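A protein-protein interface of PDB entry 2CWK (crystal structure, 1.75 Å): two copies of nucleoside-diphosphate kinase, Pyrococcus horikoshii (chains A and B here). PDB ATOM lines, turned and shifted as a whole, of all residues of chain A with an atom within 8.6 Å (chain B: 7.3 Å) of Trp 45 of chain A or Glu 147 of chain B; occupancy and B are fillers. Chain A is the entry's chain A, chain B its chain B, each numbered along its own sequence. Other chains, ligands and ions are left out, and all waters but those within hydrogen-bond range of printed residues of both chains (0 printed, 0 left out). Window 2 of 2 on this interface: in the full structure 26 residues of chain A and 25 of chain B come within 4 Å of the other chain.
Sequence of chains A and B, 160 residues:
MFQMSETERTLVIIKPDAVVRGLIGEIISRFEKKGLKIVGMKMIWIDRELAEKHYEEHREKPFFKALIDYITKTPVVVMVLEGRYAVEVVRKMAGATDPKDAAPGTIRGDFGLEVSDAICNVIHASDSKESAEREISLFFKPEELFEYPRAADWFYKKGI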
ATOM      1  N   PRO A  16       2.333 -23.787  -3.160  1.00  0.00           N
ATOM      2  CA  PRO A  16       2.471 -24.487  -4.441  1.00  0.00           C
ATOM      3  C   PRO A  16       1.385 -25.503  -4.762  1.00  0.00           C
ATOM      4  O   PRO A  16       0.948 -25.593  -5.910  1.00  0.00           O
ATOM      5  CB  PRO A  16       3.854 -25.122  -4.336  1.00  0.00           C
ATOM      6  CG  PRO A  16       4.607 -24.093  -3.558  1.00  0.00           C
ATOM      7  CD  PRO A  16       3.621 -23.778  -2.444  1.00  0.00           C
ATOM      8  N   LYS A  42       0.817 -10.608  -4.610  1.00  0.00           N
ATOM      9  CA  LYS A  42       1.677 -10.823  -5.761  1.00  0.00           C
ATOM     10  C   LYS A  42       2.109 -12.270  -5.877  1.00  0.00           C
ATOM     11  O   LYS A  42       2.220 -12.985  -4.877  1.00  0.00           O
ATOM     12  CB  LYS A  42       2.919  -9.929  -5.680  1.00  0.00           C
ATOM     13  CG  LYS A  42       3.766 -10.109  -4.430  1.00  0.00           C
ATOM     14  CD  LYS A  42       4.962  -9.161  -4.453  1.00  0.00           C
ATOM     15  CE  LYS A  42       5.769  -9.238  -3.172  1.00  0.00           C
ATOM     16  NZ  LYS A  42       6.925  -8.292  -3.185  1.00  0.00           N
ATOM     17  N   MET A  43       2.318 -12.704  -7.113  1.00  0.00           N
ATOM     18  CA  MET A  43       2.797 -14.049  -7.363  1.00  0.00           C
ATOM     19  C   MET A  43       4.314 -13.927  -7.433  1.00  0.00           C
ATOM     20  O   MET A  43       4.847 -13.088  -8.163  1.00  0.00           O
ATOM     21  CB  MET A  43       2.264 -14.595  -8.689  1.00  0.00           C
ATOM     22  CG  MET A  43       2.882 -15.935  -9.061  1.00  0.00           C
ATOM     23  SD  MET A  43       2.171 -16.695 -10.527  1.00  0.00           S
ATOM     24  CE  MET A  43       0.733 -17.524  -9.804  1.00  0.00           C
ATOM     25  N   ILE A  44       5.001 -14.747  -6.648  1.00  0.00           N
ATOM     26  CA  ILE A  44       6.455 -14.742  -6.619  1.00  0.00           C
ATOM     27  C   ILE A  44       6.926 -16.183  -6.560  1.00  0.00           C
ATOM     28  O   ILE A  44       6.136 -17.082  -6.292  1.00  0.00           O
ATOM     29  CB  ILE A  44       7.004 -14.014  -5.367  1.00  0.00           C
ATOM     30  CG1 ILE A  44       6.516 -14.713  -4.093  1.00  0.00           C
ATOM     31  CG2 ILE A  44       6.565 -12.553  -5.378  1.00  0.00           C
ATOM     32  CD1 ILE A  44       7.156 -14.189  -2.817  1.00  0.00           C
ATOM     33  N   TRP A  45       8.205 -16.404  -6.842  1.00  0.00           N
ATOM     34  CA  TRP A  45       8.755 -17.746  -6.748  1.00  0.00           C
ATOM     35  C   TRP A  45       9.841 -17.619  -5.689  1.00  0.00           C
ATOM     36  O   TRP A  45      10.923 -17.080  -5.942  1.00  0.00           O
ATOM     37  CB  TRP A  45       9.359 -18.214  -8.075  1.00  0.00           C
ATOM     38  CG  TRP A  45       9.463 -19.719  -8.162  1.00  0.00           C
ATOM     39  CD1 TRP A  45       9.679 -20.587  -7.128  1.00  0.00           C
ATOM     40  CD2 TRP A  45       9.359 -20.524  -9.344  1.00  0.00           C
ATOM     41  NE1 TRP A  45       9.713 -21.882  -7.591  1.00  0.00           N
ATOM     42  CE2 TRP A  45       9.522 -21.871  -8.948  1.00  0.00           C
ATOM     43  CE3 TRP A  45       9.146 -20.238 -10.699  1.00  0.00           C
ATOM     44  CZ2 TRP A  45       9.477 -22.932  -9.861  1.00  0.00           C
ATOM     45  CZ3 TRP A  45       9.100 -21.294 -11.607  1.00  0.00           C
ATOM     46  CH2 TRP A  45       9.265 -22.623 -11.182  1.00  0.00           C
ATOM     47  N   ILE A  46       9.525 -18.092  -4.490  1.00  0.00           N
ATOM     48  CA  ILE A  46      10.433 -18.021  -3.356  1.00  0.00           C
ATOM     49  C   ILE A  46      11.666 -18.895  -3.540  1.00  0.00           C
ATOM     50  O   ILE A  46      11.548 -20.067  -3.903  1.00  0.00           O
ATOM     51  CB  ILE A  46       9.715 -18.466  -2.063  1.00  0.00           C
ATOM     52  CG1 ILE A  46       8.467 -17.610  -1.841  1.00  0.00           C
ATOM     53  CG2 ILE A  46      10.664 -18.353  -0.871  1.00  0.00           C
ATOM     54  CD1 ILE A  46       7.583 -18.093  -0.701  1.00  0.00           C
ATOM     55  N   ASP A  47      12.848 -18.328  -3.312  1.00  0.00           N
ATOM     56  CA  ASP A  47      14.059 -19.131  -3.421  1.00  0.00           C
ATOM     57  C   ASP A  47      14.378 -19.665  -2.029  1.00  0.00           C
ATOM     58  O   ASP A  47      13.768 -19.247  -1.043  1.00  0.00           O
ATOM     59  CB  ASP A  47      15.246 -18.336  -3.997  1.00  0.00           C
ATOM     60  CG  ASP A  47      15.583 -17.088  -3.203  1.00  0.00           C
ATOM     61  OD1 ASP A  47      15.405 -17.072  -1.970  1.00  0.00           O
ATOM     62  OD2 ASP A  47      16.061 -16.116  -3.829  1.00  0.00           O
ATOM     63  N   ARG A  48      15.319 -20.594  -1.943  1.00  0.00           N
ATOM     64  CA  ARG A  48      15.647 -21.189  -0.657  1.00  0.00           C
ATOM     65  C   ARG A  48      16.021 -20.191   0.434  1.00  0.00           C
ATOM     66  O   ARG A  48      15.581 -20.333   1.571  1.00  0.00           O
ATOM     67  CB  ARG A  48      16.753 -22.238  -0.828  1.00  0.00           C
ATOM     68  CG  ARG A  48      16.399 -23.322  -1.844  1.00  0.00           C
ATOM     69  CD  ARG A  48      17.339 -24.514  -1.753  1.00  0.00           C
ATOM     70  NE  ARG A  48      17.074 -25.339  -0.577  1.00  0.00           N
ATOM     71  CZ  ARG A  48      16.091 -26.230  -0.491  1.00  0.00           C
ATOM     72  NH1 ARG A  48      15.269 -26.421  -1.514  1.00  0.00           N
ATOM     73  NH2 ARG A  48      15.926 -26.932   0.623  1.00  0.00           N
ATOM     74  N   LEU A  50      15.090 -17.027   0.889  1.00  0.00           N
ATOM     75  CA  LEU A  50      13.912 -16.321   1.383  1.00  0.00           C
ATOM     76  C   LEU A  50      13.016 -17.276   2.169  1.00  0.00           C
ATOM     77  O   LEU A  50      12.455 -16.910   3.199  1.00  0.00           O
ATOM     78  CB  LEU A  50      13.134 -15.709   0.216  1.00  0.00           C
ATOM     79  CG  LEU A  50      11.840 -14.957   0.542  1.00  0.00           C
ATOM     80  CD1 LEU A  50      12.104 -13.868   1.572  1.00  0.00           C
ATOM     81  CD2 LEU A  50      11.274 -14.356  -0.744  1.00  0.00           C
ATOM     82  N   ALA A  51      12.896 -18.504   1.676  1.00  0.00           N
ATOM     83  CA  ALA A  51      12.080 -19.512   2.342  1.00  0.00           C
ATOM     84  C   ALA A  51      12.623 -19.809   3.738  1.00  0.00           C
ATOM     85  O   ALA A  51      11.864 -19.911   4.701  1.00  0.00           O
ATOM     86  CB  ALA A  51      12.052 -20.788   1.514  1.00  0.00           C
ATOM     87  N   ILE A  68      11.228 -26.510   3.070  1.00  0.00           N
ATOM     88  CA  ILE A  68      11.785 -25.545   2.133  1.00  0.00           C
ATOM     89  C   ILE A  68      11.561 -26.038   0.706  1.00  0.00           C
ATOM     90  O   ILE A  68      11.220 -25.251  -0.177  1.00  0.00           O
ATOM     91  CB  ILE A  68      13.292 -25.324   2.390  1.00  0.00           C
ATOM     92  CG1 ILE A  68      13.506 -24.840   3.829  1.00  0.00           C
ATOM     93  CG2 ILE A  68      13.851 -24.316   1.396  1.00  0.00           C
ATOM     94  CD1 ILE A  68      12.740 -23.565   4.192  1.00  0.00           C
ATOM     95  N   ASP A  69      11.734 -27.341   0.483  1.00  0.00           N
ATOM     96  CA  ASP A  69      11.524 -27.915  -0.846  1.00  0.00           C
ATOM     97  C   ASP A  69      10.088 -27.659  -1.294  1.00  0.00           C
ATOM     98  O   ASP A  69       9.828 -27.311  -2.445  1.00  0.00           O
ATOM     99  CB  ASP A  69      11.746 -29.435  -0.849  1.00  0.00           C
ATOM    100  CG  ASP A  69      13.193 -29.830  -0.634  1.00  0.00           C
ATOM    101  OD1 ASP A  69      14.095 -29.004  -0.887  1.00  0.00           O
ATOM    102  OD2 ASP A  69      13.426 -30.990  -0.230  1.00  0.00           O
ATOM    103  N   TYR A  70       9.157 -27.847  -0.367  1.00  0.00           N
ATOM    104  CA  TYR A  70       7.738 -27.670  -0.643  1.00  0.00           C
ATOM    105  C   TYR A  70       7.354 -26.238  -0.994  1.00  0.00           C
ATOM    106  O   TYR A  70       6.752 -25.989  -2.041  1.00  0.00           O
ATOM    107  CB  TYR A  70       6.935 -28.173   0.569  1.00  0.00           C
ATOM    108  CG  TYR A  70       5.471 -27.779   0.643  1.00  0.00           C
ATOM    109  CD1 TYR A  70       4.638 -27.832  -0.478  1.00  0.00           C
ATOM    110  CD2 TYR A  70       4.909 -27.400   1.863  1.00  0.00           C
ATOM    111  CE1 TYR A  70       3.273 -27.512  -0.381  1.00  0.00           C
ATOM    112  CE2 TYR A  70       3.556 -27.085   1.975  1.00  0.00           C
ATOM    113  CZ  TYR A  70       2.744 -27.141   0.856  1.00  0.00           C
ATOM    114  OH  TYR A  70       1.412 -26.819   0.986  1.00  0.00           O
ATOM    115  N   ILE A  71       7.720 -25.293  -0.137  1.00  0.00           N
ATOM    116  CA  ILE A  71       7.351 -23.901  -0.360  1.00  0.00           C
ATOM    117  C   ILE A  71       8.014 -23.252  -1.576  1.00  0.00           C
ATOM    118  O   ILE A  71       7.543 -22.228  -2.068  1.00  0.00           O
ATOM    119  CB  ILE A  71       7.625 -23.051   0.912  1.00  0.00           C
ATOM    120  CG1 ILE A  71       6.768 -21.787   0.888  1.00  0.00           C
ATOM    121  CG2 ILE A  71       9.099 -22.700   1.013  1.00  0.00           C
ATOM    122  CD1 ILE A  71       5.277 -22.064   1.012  1.00  0.00           C
ATOM    123  N   THR A  72       9.091 -23.854  -2.073  1.00  0.00           N
ATOM    124  CA  THR A  72       9.795 -23.307  -3.235  1.00  0.00           C
ATOM    125  C   THR A  72       9.566 -24.133  -4.499  1.00  0.00           C
ATOM    126  O   THR A  72      10.182 -23.870  -5.534  1.00  0.00           O
ATOM    127  CB  THR A  72      11.317 -23.256  -2.995  1.00  0.00           C
ATOM    128  OG1 THR A  72      11.807 -24.587  -2.790  1.00  0.00           O
ATOM    129  CG2 THR A  72      11.646 -22.394  -1.777  1.00  0.00           C
ATOM    130  N   LYS A  73       8.676 -25.118  -4.422  1.00  0.00           N
ATOM    131  CA  LYS A  73       8.416 -26.003  -5.556  1.00  0.00           C
ATOM    132  C   LYS A  73       7.912 -25.297  -6.819  1.00  0.00           C
ATOM    133  O   LYS A  73       8.346 -25.616  -7.929  1.00  0.00           O
ATOM    134  CB  LYS A  73       7.441 -27.102  -5.131  1.00  0.00           C
ATOM    135  CG  LYS A  73       7.338 -28.257  -6.106  1.00  0.00           C
ATOM    136  CD  LYS A  73       6.525 -29.390  -5.503  1.00  0.00           C
ATOM    137  CE  LYS A  73       6.443 -30.580  -6.441  1.00  0.00           C
ATOM    138  NZ  LYS A  73       7.783 -31.168  -6.692  1.00  0.00           N
ATOM    139  N   THR A  74       6.992 -24.351  -6.649  1.00  0.00           N
ATOM    140  CA  THR A  74       6.445 -23.578  -7.761  1.00  0.00           C
ATOM    141  C   THR A  74       6.165 -22.170  -7.240  1.00  0.00           C
ATOM    142  O   THR A  74       6.373 -21.889  -6.057  1.00  0.00           O
ATOM    143  CB  THR A  74       5.093 -24.140  -8.260  1.00  0.00           C
ATOM    144  OG1 THR A  74       4.074 -23.852  -7.291  1.00  0.00           O
ATOM    145  CG2 THR A  74       5.172 -25.643  -8.474  1.00  0.00           C
ATOM    146  N   PRO A  75       5.719 -21.259  -8.119  1.00  0.00           N
ATOM    147  CA  PRO A  75       5.428 -19.911  -7.625  1.00  0.00           C
ATOM    148  C   PRO A  75       4.274 -20.013  -6.630  1.00  0.00           C
ATOM    149  O   PRO A  75       3.504 -20.972  -6.663  1.00  0.00           O
ATOM    150  CB  PRO A  75       4.998 -19.165  -8.886  1.00  0.00           C
ATOM    151  CG  PRO A  75       5.810 -19.826  -9.961  1.00  0.00           C
ATOM    152  CD  PRO A  75       5.717 -21.295  -9.594  1.00  0.00           C
ATOM    153  N   VAL A  76       4.166 -19.022  -5.752  1.00  0.00           N
ATOM    154  CA  VAL A  76       3.096 -18.973  -4.766  1.00  0.00           C
ATOM    155  C   VAL A  76       2.477 -17.587  -4.863  1.00  0.00           C
ATOM    156  O   VAL A  76       2.977 -16.725  -5.583  1.00  0.00           O
ATOM    157  CB  VAL A  76       3.630 -19.146  -3.321  1.00  0.00           C
ATOM    158  CG1 VAL A  76       4.238 -20.525  -3.148  1.00  0.00           C
ATOM    159  CG2 VAL A  76       4.666 -18.060  -3.008  1.00  0.00           C
ATOM    160  N   VAL A  77       1.378 -17.374  -4.154  1.00  0.00           N
ATOM    161  CA  VAL A  77       0.765 -16.058  -4.144  1.00  0.00           C
ATOM    162  C   VAL A  77       0.834 -15.591  -2.697  1.00  0.00           C
ATOM    163  O   VAL A  77       0.284 -16.230  -1.802  1.00  0.00           O
ATOM    164  CB  VAL A  77      -0.708 -16.088  -4.614  1.00  0.00           C
ATOM    165  CG1 VAL A  77      -1.323 -14.697  -4.491  1.00  0.00           C
ATOM    166  CG2 VAL A  77      -0.778 -16.545  -6.063  1.00  0.00           C
ATOM    167  N   VAL A  78       1.562 -14.507  -2.455  1.00  0.00           N
ATOM    168  CA  VAL A  78       1.649 -13.975  -1.105  1.00  0.00           C
ATOM    169  C   VAL A  78       0.686 -12.806  -1.062  1.00  0.00           C
ATOM    170  O   VAL A  78       0.600 -12.030  -2.011  1.00  0.00           O
ATOM    171  CB  VAL A  78       3.080 -13.498  -0.755  1.00  0.00           C
ATOM    172  CG1 VAL A  78       4.026 -14.690  -0.715  1.00  0.00           C
ATOM    173  CG2 VAL A  78       3.561 -12.473  -1.769  1.00  0.00           C
ATOM    174  N   PHE A 139       8.209 -10.157   2.855  1.00  0.00           N
ATOM    175  CA  PHE A 139       7.735 -10.278   1.485  1.00  0.00           C
ATOM    176  C   PHE A 139       7.302  -9.003   0.775  1.00  0.00           C
ATOM    177  O   PHE A 139       7.325  -8.947  -0.452  1.00  0.00           O
ATOM    178  CB  PHE A 139       6.576 -11.276   1.429  1.00  0.00           C
ATOM    179  CG  PHE A 139       6.972 -12.685   1.754  1.00  0.00           C
ATOM    180  CD1 PHE A 139       6.715 -13.224   3.012  1.00  0.00           C
ATOM    181  CD2 PHE A 139       7.618 -13.470   0.804  1.00  0.00           C
ATOM    182  CE1 PHE A 139       7.097 -14.532   3.319  1.00  0.00           C
ATOM    183  CE2 PHE A 139       8.004 -14.777   1.100  1.00  0.00           C
ATOM    184  CZ  PHE A 139       7.742 -15.309   2.360  1.00  0.00           C
ATOM    185  N   ARG B   9       0.094 -15.392 -24.308  1.00  0.00           N
ATOM    186  CA  ARG B   9      -0.029 -14.744 -23.014  1.00  0.00           C
ATOM    187  C   ARG B   9      -0.826 -13.472 -23.233  1.00  0.00           C
ATOM    188  O   ARG B   9      -0.618 -12.768 -24.223  1.00  0.00           O
ATOM    189  CB  ARG B   9       1.344 -14.377 -22.443  1.00  0.00           C
ATOM    190  CG  ARG B   9       2.152 -15.554 -21.929  1.00  0.00           C
ATOM    191  CD  ARG B   9       3.441 -15.066 -21.295  1.00  0.00           C
ATOM    192  NE  ARG B   9       4.180 -16.146 -20.646  1.00  0.00           N
ATOM    193  CZ  ARG B   9       5.347 -15.982 -20.030  1.00  0.00           C
ATOM    194  NH1 ARG B   9       5.909 -14.782 -19.982  1.00  0.00           N
ATOM    195  NH2 ARG B   9       5.951 -17.016 -19.457  1.00  0.00           N
ATOM    196  N   LYS B  37      -3.362 -20.518 -17.225  1.00  0.00           N
ATOM    197  CA  LYS B  37      -2.336 -20.458 -16.194  1.00  0.00           C
ATOM    198  C   LYS B  37      -1.940 -19.027 -15.857  1.00  0.00           C
ATOM    199  O   LYS B  37      -1.693 -18.214 -16.747  1.00  0.00           O
ATOM    200  CB  LYS B  37      -1.101 -21.234 -16.669  1.00  0.00           C
ATOM    201  CG  LYS B  37       0.075 -21.241 -15.699  1.00  0.00           C
ATOM    202  CD  LYS B  37       1.286 -21.936 -16.324  1.00  0.00           C
ATOM    203  CE  LYS B  37       0.984 -23.386 -16.661  1.00  0.00           C
ATOM    204  NZ  LYS B  37       2.123 -24.048 -17.367  1.00  0.00           N
ATOM    205  N   VAL B  39       0.705 -16.694 -14.912  1.00  0.00           N
ATOM    206  CA  VAL B  39       2.162 -16.691 -14.899  1.00  0.00           C
ATOM    207  C   VAL B  39       2.727 -15.435 -14.253  1.00  0.00           C
ATOM    208  O   VAL B  39       3.934 -15.315 -14.057  1.00  0.00           O
ATOM    209  CB  VAL B  39       2.739 -16.849 -16.323  1.00  0.00           C
ATOM    210  CG1 VAL B  39       2.305 -18.190 -16.902  1.00  0.00           C
ATOM    211  CG2 VAL B  39       2.281 -15.702 -17.212  1.00  0.00           C
ATOM    212  N   GLU B  82      -1.734 -17.392 -19.385  1.00  0.00           N
ATOM    213  CA  GLU B  82      -1.101 -18.135 -20.464  1.00  0.00           C
ATOM    214  C   GLU B  82      -1.922 -19.360 -20.846  1.00  0.00           C
ATOM    215  O   GLU B  82      -2.422 -20.079 -19.979  1.00  0.00           O
ATOM    216  CB  GLU B  82       0.302 -18.569 -20.035  1.00  0.00           C
ATOM    217  CG  GLU B  82       1.114 -19.264 -21.113  1.00  0.00           C
ATOM    218  CD  GLU B  82       2.538 -19.531 -20.664  1.00  0.00           C
ATOM    219  OE1 GLU B  82       2.742 -20.420 -19.809  1.00  0.00           O
ATOM    220  OE2 GLU B  82       3.455 -18.841 -21.159  1.00  0.00           O
ATOM    221  N   GLU B 143      11.361 -10.785 -14.650  1.00  0.00           N
ATOM    222  CA  GLU B 143      11.551 -11.515 -13.401  1.00  0.00           C
ATOM    223  C   GLU B 143      10.251 -11.766 -12.645  1.00  0.00           C
ATOM    224  O   GLU B 143      10.229 -12.528 -11.680  1.00  0.00           O
ATOM    225  CB  GLU B 143      12.527 -10.762 -12.493  1.00  0.00           C
ATOM    226  CG  GLU B 143      13.961 -10.746 -13.001  1.00  0.00           C
ATOM    227  CD  GLU B 143      14.872  -9.871 -12.159  1.00  0.00           C
ATOM    228  OE1 GLU B 143      14.975 -10.114 -10.937  1.00  0.00           O
ATOM    229  OE2 GLU B 143      15.488  -8.941 -12.723  1.00  0.00           O
ATOM    230  N   LEU B 145       7.454 -12.888 -14.216  1.00  0.00           N
ATOM    231  CA  LEU B 145       6.680 -13.855 -14.989  1.00  0.00           C
ATOM    232  C   LEU B 145       7.342 -15.218 -14.838  1.00  0.00           C
ATOM    233  O   LEU B 145       8.565 -15.337 -14.941  1.00  0.00           O
ATOM    234  CB  LEU B 145       6.635 -13.428 -16.457  1.00  0.00           C
ATOM    235  CG  LEU B 145       6.075 -12.018 -16.670  1.00  0.00           C
ATOM    236  CD1 LEU B 145       6.194 -11.634 -18.135  1.00  0.00           C
ATOM    237  CD2 LEU B 145       4.618 -11.960 -16.212  1.00  0.00           C
ATOM    238  N   PHE B 146       6.536 -16.253 -14.615  1.00  0.00           N
ATOM    239  CA  PHE B 146       7.094 -17.579 -14.380  1.00  0.00           C
ATOM    240  C   PHE B 146       6.645 -18.713 -15.291  1.00  0.00           C
ATOM    241  O   PHE B 146       5.563 -18.682 -15.878  1.00  0.00           O
ATOM    242  CB  PHE B 146       6.818 -17.980 -12.927  1.00  0.00           C
ATOM    243  CG  PHE B 146       7.118 -16.892 -11.934  1.00  0.00           C
ATOM    244  CD1 PHE B 146       6.109 -16.040 -11.486  1.00  0.00           C
ATOM    245  CD2 PHE B 146       8.415 -16.697 -11.476  1.00  0.00           C
ATOM    246  CE1 PHE B 146       6.391 -15.005 -10.592  1.00  0.00           C
ATOM    247  CE2 PHE B 146       8.710 -15.669 -10.584  1.00  0.00           C
ATOM    248  CZ  PHE B 146       7.695 -14.820 -10.140  1.00  0.00           C
ATOM    249  N   GLU B 147       7.506 -19.722 -15.386  1.00  0.00           N
ATOM    250  CA  GLU B 147       7.251 -20.919 -16.173  1.00  0.00           C
ATOM    251  C   GLU B 147       7.206 -22.060 -15.164  1.00  0.00           C
ATOM    252  O   GLU B 147       8.224 -22.399 -14.555  1.00  0.00           O
ATOM    253  CB  GLU B 147       8.391 -21.151 -17.170  1.00  0.00           C
ATOM    254  CG  GLU B 147       8.241 -22.392 -18.030  1.00  0.00           C
ATOM    255  CD  GLU B 147       7.013 -22.345 -18.917  1.00  0.00           C
ATOM    256  OE1 GLU B 147       6.835 -21.338 -19.637  1.00  0.00           O
ATOM    257  OE2 GLU B 147       6.232 -23.321 -18.903  1.00  0.00           O
ATOM    258  N   TYR B 148       6.027 -22.640 -14.975  1.00  0.00           N
ATOM    259  CA  TYR B 148       5.866 -23.725 -14.023  1.00  0.00           C
ATOM    260  C   TYR B 148       4.692 -24.593 -14.449  1.00  0.00           C
ATOM    261  O   TYR B 148       3.830 -24.164 -15.209  1.00  0.00           O
ATOM    262  CB  TYR B 148       5.620 -23.156 -12.623  1.00  0.00           C
ATOM    263  CG  TYR B 148       4.292 -22.455 -12.490  1.00  0.00           C
ATOM    264  CD1 TYR B 148       3.171 -23.133 -12.010  1.00  0.00           C
ATOM    265  CD2 TYR B 148       4.143 -21.125 -12.880  1.00  0.00           C
ATOM    266  CE1 TYR B 148       1.933 -22.504 -11.923  1.00  0.00           C
ATOM    267  CE2 TYR B 148       2.908 -20.484 -12.798  1.00  0.00           C
ATOM    268  CZ  TYR B 148       1.808 -21.181 -12.318  1.00  0.00           C
ATOM    269  OH  TYR B 148       0.585 -20.559 -12.230  1.00  0.00           O
ATOM    270  N   PRO B 149       4.637 -25.829 -13.946  1.00  0.00           N
ATOM    271  CA  PRO B 149       3.544 -26.726 -14.314  1.00  0.00           C
ATOM    272  C   PRO B 149       2.258 -26.603 -13.507  1.00  0.00           C
ATOM    273  O   PRO B 149       2.288 -26.494 -12.278  1.00  0.00           O
ATOM    274  CB  PRO B 149       4.174 -28.100 -14.134  1.00  0.00           C
ATOM    275  CG  PRO B 149       5.019 -27.885 -12.912  1.00  0.00           C
ATOM    276  CD  PRO B 149       5.683 -26.550 -13.198  1.00  0.00           C
ATOM    277  N   ASP B 153      -1.053 -30.183 -16.777  1.00  0.00           N
ATOM    278  CA  ASP B 153      -0.216 -29.928 -17.948  1.00  0.00           C
ATOM    279  C   ASP B 153       0.256 -31.212 -18.639  1.00  0.00           C
ATOM    280  O   ASP B 153       0.267 -31.287 -19.872  1.00  0.00           O
ATOM    281  CB  ASP B 153       1.003 -29.076 -17.568  1.00  0.00           C
ATOM    282  CG  ASP B 153       0.656 -27.609 -17.358  1.00  0.00           C
ATOM    283  OD1 ASP B 153      -0.542 -27.255 -17.428  1.00  0.00           O
ATOM    284  OD2 ASP B 153       1.587 -26.809 -17.119  1.00  0.00           O
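No position is printed for both chains.
Of the 9 pairs that touch across the chains among the printed residues, none has its exchanged pair printed and touching as well.
O of Ile 44 of chain A sits at hydrogen-bond distance from N of Val 76 of chain A (2.8 Å).
The backbone carbonyl oxygen of Val 39 of chain B is in hydrogen-bond range of the backbone NH of Phe 146 of chain B (2.8 Å).
NE1 of Trp 45 of chain A sits at hydrogen-bond distance from O of Thr 72 of chain A.
The side-chain amino group (NZ) of Lys 37 of chain B sits at hydrogen-bond distance from the backbone carbonyl oxygen (O) of Tyr 148 of chain B (2.8 Å).
Among the printed residues, merely in contact across the chains: Met 43 of chain A with Val 39 of chain B (3.97 Å), Met 43 of chain A with Phe 146 of chain B (3.5 Å), Met 43 of chain A with Tyr 148 of chain B (3.9 Å), Ile 44 of chain A with Phe 146 of chain B (3.7 Å), Trp 45 of chain A with Phe 146 of chain B (3.6 Å), Trp 45 of chain A with Glu 147 of chain B (3.3 Å), Trp 45 of chain A with Tyr 148 of chain B (3.96 Å), Pro 75 of chain A with Phe 146 of chain B (3.6 Å) and Pro 75 of chain A with Tyr 148 of chain B (3.4 Å).
Among the printed residues, no Asp or Glu carboxylate lies within 4 Å of a Lys or Arg side-chain nitrogen of the other chain.
Of the printed residues of chain B, Trp 45 of chain A touches Phe 146 (3.6 Å), Glu 147 (3.3 Å) and Tyr 148 (3.96 Å).
Of chain A, only Trp 45 comes within 4 Å of Glu 147 of chain B.
Printed residues of chain B within 4 Å of Pro 75 of chain A: Phe 146 and Tyr 148.
Printed residues of chain A within 4 Å of Val 39 of chain B: Met 43.
Of the printed residues of chain A, Phe 146 of chain B touches Met 43 (3.5 Å), Ile 44 (3.7 Å), Trp 45 (3.6 Å) and Pro 75 (3.6 Å).
Printed residues of chain B within 4 Å of Ile 44 of chain A: Phe 146.
Of the printed residues of chain A, Tyr 148 of chain B touches Met 43, Trp 45 and Pro 75.
The nearest residue of chain B that does not touch Trp 45 of chain A is Pro 149 of chain B (5.7 Å).
The nearest residue of chain A that does not touch Glu 147 of chain B is Pro 75 of chain A (5.7 Å).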
